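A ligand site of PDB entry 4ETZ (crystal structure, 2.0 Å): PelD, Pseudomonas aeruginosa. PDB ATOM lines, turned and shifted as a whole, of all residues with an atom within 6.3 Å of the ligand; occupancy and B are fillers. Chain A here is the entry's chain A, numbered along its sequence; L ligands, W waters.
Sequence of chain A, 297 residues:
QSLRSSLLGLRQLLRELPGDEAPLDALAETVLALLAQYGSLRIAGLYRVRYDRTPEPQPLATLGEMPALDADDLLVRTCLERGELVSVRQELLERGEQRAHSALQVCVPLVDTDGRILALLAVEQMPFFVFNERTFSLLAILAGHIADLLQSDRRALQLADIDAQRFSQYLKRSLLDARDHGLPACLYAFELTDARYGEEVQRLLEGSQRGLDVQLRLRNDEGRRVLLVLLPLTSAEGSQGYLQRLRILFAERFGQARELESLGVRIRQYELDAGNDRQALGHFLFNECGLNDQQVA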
ATOM      1  N   GLN A   1      13.479  -4.534 -10.446  1.00  0.00           N
ATOM      2  CA  GLN A   1      14.692  -4.105 -11.207  1.00  0.00           C
ATOM      3  C   GLN A   1      15.261  -5.264 -12.027  1.00  0.00           C
ATOM      4  O   GLN A   1      15.950  -5.054 -13.011  1.00  0.00           O
ATOM      5  CB  GLN A   1      15.756  -3.528 -10.260  1.00  0.00           C
ATOM      6  CG  GLN A   1      17.004  -3.006 -10.992  1.00  0.00           C
ATOM      7  CD  GLN A   1      17.333  -1.570 -10.599  1.00  0.00           C
ATOM      8  OE1 GLN A   1      17.696  -1.300  -9.455  1.00  0.00           O
ATOM      9  NE2 GLN A   1      17.214  -0.643 -11.556  1.00  0.00           N
ATOM     10  N   ARG A   4      13.494  -5.283 -15.513  1.00  0.00           N
ATOM     11  CA  ARG A   4      14.056  -4.182 -16.293  1.00  0.00           C
ATOM     12  C   ARG A   4      15.468  -4.499 -16.819  1.00  0.00           C
ATOM     13  O   ARG A   4      15.748  -4.307 -18.007  1.00  0.00           O
ATOM     14  CB  ARG A   4      14.006  -2.834 -15.525  1.00  0.00           C
ATOM     15  CG  ARG A   4      12.561  -2.358 -15.254  1.00  0.00           C
ATOM     16  CD  ARG A   4      12.442  -0.834 -14.948  1.00  0.00           C
ATOM     17  NE  ARG A   4      13.267  -0.350 -13.831  1.00  0.00           N
ATOM     18  CZ  ARG A   4      13.125  -0.671 -12.548  1.00  0.00           C
ATOM     19  NH1 ARG A   4      12.192  -1.523 -12.147  1.00  0.00           N
ATOM     20  NH2 ARG A   4      13.947  -0.136 -11.638  1.00  0.00           N
ATOM     21  N   SER A 208      19.484  12.973 -19.216  1.00  0.00           N
ATOM     22  CA  SER A 208      19.133  12.171 -18.039  1.00  0.00           C
ATOM     23  C   SER A 208      18.464  10.814 -18.349  1.00  0.00           C
ATOM     24  O   SER A 208      18.290  10.000 -17.428  1.00  0.00           O
ATOM     25  CB  SER A 208      18.170  12.931 -17.120  1.00  0.00           C
ATOM     26  OG  SER A 208      16.895  12.974 -17.704  1.00  0.00           O
ATOM     27  N   GLN A 209      18.034  10.609 -19.597  1.00  0.00           N
ATOM     28  CA  GLN A 209      17.323   9.369 -19.969  1.00  0.00           C
ATOM     29  C   GLN A 209      18.080   8.112 -19.527  1.00  0.00           C
ATOM     30  O   GLN A 209      19.262   8.003 -19.774  1.00  0.00           O
ATOM     31  CB  GLN A 209      17.014   9.317 -21.479  1.00  0.00           C
ATOM     32  CG  GLN A 209      16.121   8.129 -21.790  1.00  0.00           C
ATOM     33  CD  GLN A 209      15.908   7.895 -23.257  1.00  0.00           C
ATOM     34  OE1 GLN A 209      15.155   8.621 -23.925  1.00  0.00           O
ATOM     35  NE2 GLN A 209      16.528   6.841 -23.778  1.00  0.00           N
ATOM     36  N   ARG A 210      17.389   7.190 -18.839  1.00  0.00           N
ATOM     37  CA  ARG A 210      18.026   6.032 -18.223  1.00  0.00           C
ATOM     38  C   ARG A 210      17.236   4.744 -18.539  1.00  0.00           C
ATOM     39  O   ARG A 210      16.020   4.740 -18.481  1.00  0.00           O
ATOM     40  CB  ARG A 210      18.058   6.219 -16.689  1.00  0.00           C
ATOM     41  CG  ARG A 210      18.913   5.181 -15.952  1.00  0.00           C
ATOM     42  CD  ARG A 210      18.958   5.429 -14.443  1.00  0.00           C
ATOM     43  NE  ARG A 210      20.043   6.323 -14.039  1.00  0.00           N
ATOM     44  CZ  ARG A 210      20.339   6.616 -12.777  1.00  0.00           C
ATOM     45  NH1 ARG A 210      19.644   6.084 -11.758  1.00  0.00           N
ATOM     46  NH2 ARG A 210      21.351   7.423 -12.525  1.00  0.00           N
ATOM     47  N   GLY A 211      17.936   3.646 -18.845  1.00  0.00           N
ATOM     48  CA  GLY A 211      17.274   2.319 -18.894  1.00  0.00           C
ATOM     49  C   GLY A 211      16.175   2.250 -19.944  1.00  0.00           C
ATOM     50  O   GLY A 211      16.356   2.684 -21.066  1.00  0.00           O
ATOM     51  N   ASP A 213      13.374   3.936 -19.894  1.00  0.00           N
ATOM     52  CA  ASP A 213      12.667   5.196 -20.104  1.00  0.00           C
ATOM     53  C   ASP A 213      12.741   5.682 -21.532  1.00  0.00           C
ATOM     54  O   ASP A 213      13.792   5.593 -22.176  1.00  0.00           O
ATOM     55  CB  ASP A 213      13.191   6.276 -19.144  1.00  0.00           C
ATOM     56  CG  ASP A 213      13.011   5.881 -17.697  1.00  0.00           C
ATOM     57  OD1 ASP A 213      12.377   4.816 -17.404  1.00  0.00           O
ATOM     58  OD2 ASP A 213      13.520   6.628 -16.840  1.00  0.00           O
ATOM     59  N   LEU A 230       8.275   8.712 -20.261  1.00  0.00           N
ATOM     60  CA  LEU A 230       7.575   7.530 -19.746  1.00  0.00           C
ATOM     61  C   LEU A 230       8.556   6.704 -18.974  1.00  0.00           C
ATOM     62  O   LEU A 230       9.644   6.427 -19.486  1.00  0.00           O
ATOM     63  CB  LEU A 230       7.013   6.709 -20.902  1.00  0.00           C
ATOM     64  CG  LEU A 230       6.425   5.326 -20.500  1.00  0.00           C
ATOM     65  CD1 LEU A 230       5.121   5.521 -19.677  1.00  0.00           C
ATOM     66  CD2 LEU A 230       6.154   4.493 -21.782  1.00  0.00           C
ATOM     67  N   LEU A 231       8.197   6.343 -17.746  1.00  0.00           N
ATOM     68  CA  LEU A 231       8.999   5.491 -16.885  1.00  0.00           C
ATOM     69  C   LEU A 231       8.312   4.100 -16.767  1.00  0.00           C
ATOM     70  O   LEU A 231       7.511   3.880 -15.839  1.00  0.00           O
ATOM     71  CB  LEU A 231       9.169   6.113 -15.460  1.00  0.00           C
ATOM     72  CG  LEU A 231       9.620   7.580 -15.202  1.00  0.00           C
ATOM     73  CD1 LEU A 231       9.998   7.780 -13.712  1.00  0.00           C
ATOM     74  CD2 LEU A 231      10.754   7.942 -16.051  1.00  0.00           C
ATOM     75  N   PRO A 232       8.628   3.159 -17.693  1.00  0.00           N
ATOM     76  CA  PRO A 232       8.042   1.809 -17.635  1.00  0.00           C
ATOM     77  C   PRO A 232       8.392   1.113 -16.364  1.00  0.00           C
ATOM     78  O   PRO A 232       9.488   1.283 -15.851  1.00  0.00           O
ATOM     79  CB  PRO A 232       8.717   1.044 -18.830  1.00  0.00           C
ATOM     80  CG  PRO A 232       9.181   2.116 -19.735  1.00  0.00           C
ATOM     81  CD  PRO A 232       9.484   3.336 -18.899  1.00  0.00           C
ATOM     82  N   LEU A 233       7.471   0.301 -15.852  1.00  0.00           N
ATOM     83  CA  LEU A 233       7.773  -0.630 -14.753  1.00  0.00           C
ATOM     84  C   LEU A 233       8.397   0.056 -13.546  1.00  0.00           C
ATOM     85  O   LEU A 233       9.356  -0.440 -12.936  1.00  0.00           O
ATOM     86  CB  LEU A 233       8.664  -1.800 -15.234  1.00  0.00           C
ATOM     87  CG  LEU A 233       8.161  -2.605 -16.443  1.00  0.00           C
ATOM     88  CD1 LEU A 233       9.276  -3.432 -17.063  1.00  0.00           C
ATOM     89  CD2 LEU A 233       6.984  -3.511 -16.031  1.00  0.00           C
ATOM     90  N   THR A 234       7.814   1.195 -13.189  1.00  0.00           N
ATOM     91  CA  THR A 234       8.326   2.051 -12.135  1.00  0.00           C
ATOM     92  C   THR A 234       7.186   2.422 -11.192  1.00  0.00           C
ATOM     93  O   THR A 234       6.112   2.836 -11.645  1.00  0.00           O
ATOM     94  CB  THR A 234       8.975   3.320 -12.766  1.00  0.00           C
ATOM     95  OG1 THR A 234      10.079   2.905 -13.573  1.00  0.00           O
ATOM     96  CG2 THR A 234       9.476   4.307 -11.675  1.00  0.00           C
ATOM     97  N   SER A 235       7.395   2.255  -9.892  1.00  0.00           N
ATOM     98  CA  SER A 235       6.358   2.495  -8.890  1.00  0.00           C
ATOM     99  C   SER A 235       6.370   3.971  -8.525  1.00  0.00           C
ATOM    100  O   SER A 235       7.254   4.719  -8.959  1.00  0.00           O
ATOM    101  CB  SER A 235       6.643   1.652  -7.663  1.00  0.00           C
ATOM    102  OG  SER A 235       7.957   1.974  -7.200  1.00  0.00           O
ATOM    103  N   GLU A 237       7.060   5.187  -5.598  1.00  0.00           N
ATOM    104  CA  GLU A 237       8.374   5.378  -5.030  1.00  0.00           C
ATOM    105  C   GLU A 237       9.246   5.114  -6.257  1.00  0.00           C
ATOM    106  O   GLU A 237       8.900   4.322  -7.114  1.00  0.00           O
ATOM    107  CB  GLU A 237       8.639   4.374  -3.925  1.00  0.00           C
ATOM    108  CG  GLU A 237       8.230   2.911  -4.298  1.00  0.00           C
ATOM    109  CD  GLU A 237       6.822   2.445  -3.788  1.00  0.00           C
ATOM    110  OE1 GLU A 237       5.773   2.741  -4.434  1.00  0.00           O
ATOM    111  OE2 GLU A 237       6.780   1.723  -2.769  1.00  0.00           O
ATOM    112  N   GLY A 238      10.353   5.761  -6.437  1.00  0.00           N
ATOM    113  CA  GLY A 238      10.926   5.399  -7.756  1.00  0.00           C
ATOM    114  C   GLY A 238      10.631   6.531  -8.727  1.00  0.00           C
ATOM    115  O   GLY A 238      11.559   7.132  -9.207  1.00  0.00           O
ATOM    116  N   SER A 239       9.358   6.815  -9.011  1.00  0.00           N
ATOM    117  CA  SER A 239       8.999   8.050  -9.726  1.00  0.00           C
ATOM    118  C   SER A 239       9.491   9.237  -8.920  1.00  0.00           C
ATOM    119  O   SER A 239      10.027  10.204  -9.456  1.00  0.00           O
ATOM    120  CB  SER A 239       7.487   8.190  -9.898  1.00  0.00           C
ATOM    121  OG  SER A 239       7.023   7.176 -10.745  1.00  0.00           O
ATOM    122  N   GLN A 240       9.322   9.155  -7.608  1.00  0.00           N
ATOM    123  CA  GLN A 240       9.748  10.246  -6.788  1.00  0.00           C
ATOM    124  C   GLN A 240      11.294  10.240  -6.671  1.00  0.00           C
ATOM    125  O   GLN A 240      11.931  11.304  -6.590  1.00  0.00           O
ATOM    126  CB  GLN A 240       8.989  10.239  -5.453  1.00  0.00           C
ATOM    127  CG  GLN A 240       7.414  10.313  -5.638  1.00  0.00           C
ATOM    128  CD  GLN A 240       6.872  11.711  -6.030  1.00  0.00           C
ATOM    129  OE1 GLN A 240       6.097  11.833  -6.974  1.00  0.00           O
ATOM    130  NE2 GLN A 240       7.277  12.750  -5.301  1.00  0.00           N
ATOM    131  N   GLY A 241      11.874   9.039  -6.707  1.00  0.00           N
ATOM    132  CA  GLY A 241      13.298   8.881  -6.752  1.00  0.00           C
ATOM    133  C   GLY A 241      13.884   9.484  -8.041  1.00  0.00           C
ATOM    134  O   GLY A 241      14.950  10.036  -7.993  1.00  0.00           O
ATOM    135  N   TYR A 242      13.153   9.371  -9.148  1.00  0.00           N
ATOM    136  CA  TYR A 242      13.507   9.982 -10.436  1.00  0.00           C
ATOM    137  C   TYR A 242      13.530  11.491 -10.385  1.00  0.00           C
ATOM    138  O   TYR A 242      14.494  12.105 -10.828  1.00  0.00           O
ATOM    139  CB  TYR A 242      12.503   9.541 -11.506  1.00  0.00           C
ATOM    140  CG  TYR A 242      12.631  10.242 -12.826  1.00  0.00           C
ATOM    141  CD1 TYR A 242      13.831  10.188 -13.586  1.00  0.00           C
ATOM    142  CD2 TYR A 242      11.557  10.978 -13.322  1.00  0.00           C
ATOM    143  CE1 TYR A 242      13.936  10.856 -14.803  1.00  0.00           C
ATOM    144  CE2 TYR A 242      11.637  11.643 -14.523  1.00  0.00           C
ATOM    145  CZ  TYR A 242      12.830  11.568 -15.277  1.00  0.00           C
ATOM    146  OH  TYR A 242      12.885  12.211 -16.483  1.00  0.00           O
ATOM    147  N   LEU A 243      12.446  12.090  -9.858  1.00  0.00           N
ATOM    148  CA  LEU A 243      12.377  13.529  -9.739  1.00  0.00           C
ATOM    149  C   LEU A 243      13.433  14.046  -8.758  1.00  0.00           C
ATOM    150  O   LEU A 243      14.022  15.096  -8.995  1.00  0.00           O
ATOM    151  CB  LEU A 243      10.971  13.988  -9.396  1.00  0.00           C
ATOM    152  CG  LEU A 243      10.578  15.478  -9.385  1.00  0.00           C
ATOM    153  CD1 LEU A 243      11.268  16.341 -10.470  1.00  0.00           C
ATOM    154  CD2 LEU A 243       9.085  15.570  -9.519  1.00  0.00           C
ATOM    155  N   ARG A 245      16.470  12.651  -8.234  1.00  0.00           N
ATOM    156  CA  ARG A 245      17.711  12.620  -9.036  1.00  0.00           C
ATOM    157  C   ARG A 245      17.767  13.825  -9.985  1.00  0.00           C
ATOM    158  O   ARG A 245      18.803  14.495 -10.105  1.00  0.00           O
ATOM    159  CB  ARG A 245      17.789  11.325  -9.863  1.00  0.00           C
ATOM    160  CG  ARG A 245      19.110  11.171 -10.567  1.00  0.00           C
ATOM    161  CD  ARG A 245      19.324   9.778 -11.104  1.00  0.00           C
ATOM    162  NE  ARG A 245      18.494   9.494 -12.254  1.00  0.00           N
ATOM    163  CZ  ARG A 245      18.711   9.882 -13.507  1.00  0.00           C
ATOM    164  NH1 ARG A 245      19.783  10.606 -13.849  1.00  0.00           N
ATOM    165  NH2 ARG A 245      17.840   9.533 -14.443  1.00  0.00           N
HETATM  166  P1  LIG L   1      19.405   6.877  -7.730  1.00  0.00           P
HETATM  167  O1  LIG L   1      19.575   7.893  -6.620  1.00  0.00           O
HETATM  168  O2  LIG L   1      19.858   7.247  -9.120  1.00  0.00           O
HETATM  169  O3  LIG L   1      17.906   6.396  -7.899  1.00  0.00           O
HETATM  170  C1  LIG L   1      17.097   5.943  -6.805  1.00  0.00           C
HETATM  171  C2  LIG L   1      15.789   5.361  -7.330  1.00  0.00           C
HETATM  172  O4  LIG L   1      15.100   6.344  -8.081  1.00  0.00           O
HETATM  173  C3  LIG L   1      15.966   4.227  -8.343  1.00  0.00           C
HETATM  174  O5  LIG L   1      16.135   2.935  -7.786  1.00  0.00           O
HETATM  175  C4  LIG L   1      14.736   4.277  -9.213  1.00  0.00           C
HETATM  176  O6  LIG L   1      13.692   3.473  -8.667  1.00  0.00           O
HETATM  177  C5  LIG L   1      14.394   5.751  -9.201  1.00  0.00           C
HETATM  178  N1  LIG L   1      14.940   6.380 -10.439  1.00  0.00           N
HETATM  179  C6  LIG L   1      15.972   7.230 -10.434  1.00  0.00           C
HETATM  180  N2  LIG L   1      16.248   7.704 -11.660  1.00  0.00           N
HETATM  181  C7  LIG L   1      15.377   7.104 -12.508  1.00  0.00           C
HETATM  182  C8  LIG L   1      15.110   7.125 -13.965  1.00  0.00           C
HETATM  183  O7  LIG L   1      15.827   7.889 -14.832  1.00  0.00           O
HETATM  184  N3  LIG L   1      14.081   6.368 -14.428  1.00  0.00           N
HETATM  185  C9  LIG L   1      13.318   5.550 -13.636  1.00  0.00           C
HETATM  186  N4  LIG L   1      12.335   4.827 -14.205  1.00  0.00           N
HETATM  187  N5  LIG L   1      13.494   5.500 -12.297  1.00  0.00           N
HETATM  188  C10 LIG L   1      14.499   6.234 -11.695  1.00  0.00           C
HETATM  189  P2  LIG L   1      17.020   1.836  -8.547  1.00  0.00           P
HETATM  190  O8  LIG L   1      16.893   0.575  -7.728  1.00  0.00           O
HETATM  191  O9  LIG L   1      16.632   1.756 -10.000  1.00  0.00           O
HETATM  192  O10 LIG L   1      18.499   2.406  -8.395  1.00  0.00           O
HETATM  193  C11 LIG L   1      19.134   2.470  -7.134  1.00  0.00           C
HETATM  194  C12 LIG L   1      20.468   3.118  -7.373  1.00  0.00           C
HETATM  195  O11 LIG L   1      21.172   2.315  -8.318  1.00  0.00           O
HETATM  196  C13 LIG L   1      20.360   4.447  -8.083  1.00  0.00           C
HETATM  197  O12 LIG L   1      20.178   5.551  -7.222  1.00  0.00           O
HETATM  198  C14 LIG L   1      21.679   4.574  -8.802  1.00  0.00           C
HETATM  199  O13 LIG L   1      22.721   5.020  -7.941  1.00  0.00           O
HETATM  200  C15 LIG L   1      21.955   3.146  -9.186  1.00  0.00           C
HETATM  201  N6  LIG L   1      21.489   2.978 -10.568  1.00  0.00           N
HETATM  202  C16 LIG L   1      20.349   2.360 -10.926  1.00  0.00           C
HETATM  203  N7  LIG L   1      20.208   2.363 -12.275  1.00  0.00           N
HETATM  204  C17 LIG L   1      21.273   3.017 -12.778  1.00  0.00           C
HETATM  205  C18 LIG L   1      21.729   3.358 -14.133  1.00  0.00           C
HETATM  206  O14 LIG L   1      20.975   2.970 -15.170  1.00  0.00           O
HETATM  207  N8  LIG L   1      22.856   4.057 -14.293  1.00  0.00           N
HETATM  208  C19 LIG L   1      23.606   4.413 -13.214  1.00  0.00           C
HETATM  209  N9  LIG L   1      24.751   5.094 -13.421  1.00  0.00           N
HETATM  210  N10 LIG L   1      23.239   4.112 -11.936  1.00  0.00           N
HETATM  211  C20 LIG L   1      22.113   3.423 -11.667  1.00  0.00           C
HETATM  212  O   HOH W   1      16.865   9.584  -6.014  1.00  0.00           O
HETATM  213  O   HOH W   2      24.627   3.091 -17.140  1.00  0.00           O
HETATM  214  O   HOH W   3      22.053   8.300  -9.732  1.00  0.00           O
HETATM  215  O   HOH W   4      17.232   4.030 -11.776  1.00  0.00           O
HETATM  216  O   HOH W   5      14.975   8.595 -17.495  1.00  0.00           O
HETATM  217  O   HOH W   6      12.266   1.973 -12.942  1.00  0.00           O
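Water W3 bridges O2 of the ligand and NH2 of Arg 210. Water W5 lies within hydrogen-bond range of the side-chain carboxylate (OD2) of Asp 213, an oxygen (O7) of the ligand and the backbone NH (N) of Arg 210. Water W4 lies within hydrogen-bond range of an oxygen (O9) of the ligand (2.9 Å) and the guanidinium group of Arg 210 (3.2 Å). Water W6 lies within hydrogen-bond range of the side-chain hydroxyl of Thr 234 (2.5 Å), the guanidinium group of Arg 4 (2.7 Å) and a nitrogen (N4) of the ligand (3.1 Å). Water W1 lies within hydrogen-bond range of the backbone carbonyl oxygen of Gly 241 (2.8 Å) and an oxygen (O1) of the ligand (3.3 Å).
The backbone carbonyl oxygen of Asp 213 sits close to the side-chain amide nitrogen of Gln 209. The guanidinium group (NH2) of Arg 245 sits at hydrogen-bond distance from the backbone carbonyl oxygen (O) of Ser 208, 3.1 Å away. The side-chain amide nitrogen of Gln 1 sits close to the guanidinium group of Arg 4, 3.3 Å away. The side-chain hydroxyl of Thr 234 sits at hydrogen-bond distance from the backbone carbonyl oxygen of Pro 232, at 2.9 Å. The backbone carbonyl oxygen (O) of Leu 233 is in hydrogen-bond range of the guanidinium group (NH1) of Arg 4 (3.1 Å).
OD2 of Asp 213 is in hydrogen-bond range of N3 of the ligand (2.5 Å). O7 of the ligand sits at hydrogen-bond distance from NH2 of Arg 245 (2.6 Å). The side-chain amide oxygen of Gln 1 sits close to an oxygen (O8) of the ligand (2.7 Å). O2 of the ligand lies within salt-bridge range of NH1 of Arg 210. OG1 of Thr 234 is in hydrogen-bond range of N4 of the ligand (3.0 Å). The guanidinium group of Arg 4 lies within salt-bridge range of an oxygen (O9) of the ligand.
Residues that only touch the ligand: Leu 231 (3.6 Å), Gly 238 (3.2 Å), Gly 241 (3.4 Å) and Tyr 242 (3.3 Å). Within 4 Å of the ligand: Gln 1, Arg 4, Arg 210, Asp 213, Leu 231, Thr 234, Gly 238, Gly 241, Tyr 242 and Arg 245. Along chain A the residues within 4 Å of the ligand span positions 1 to 245. The nearest printed residue that does not touch the ligand is Ser 208 (4.2 Å).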
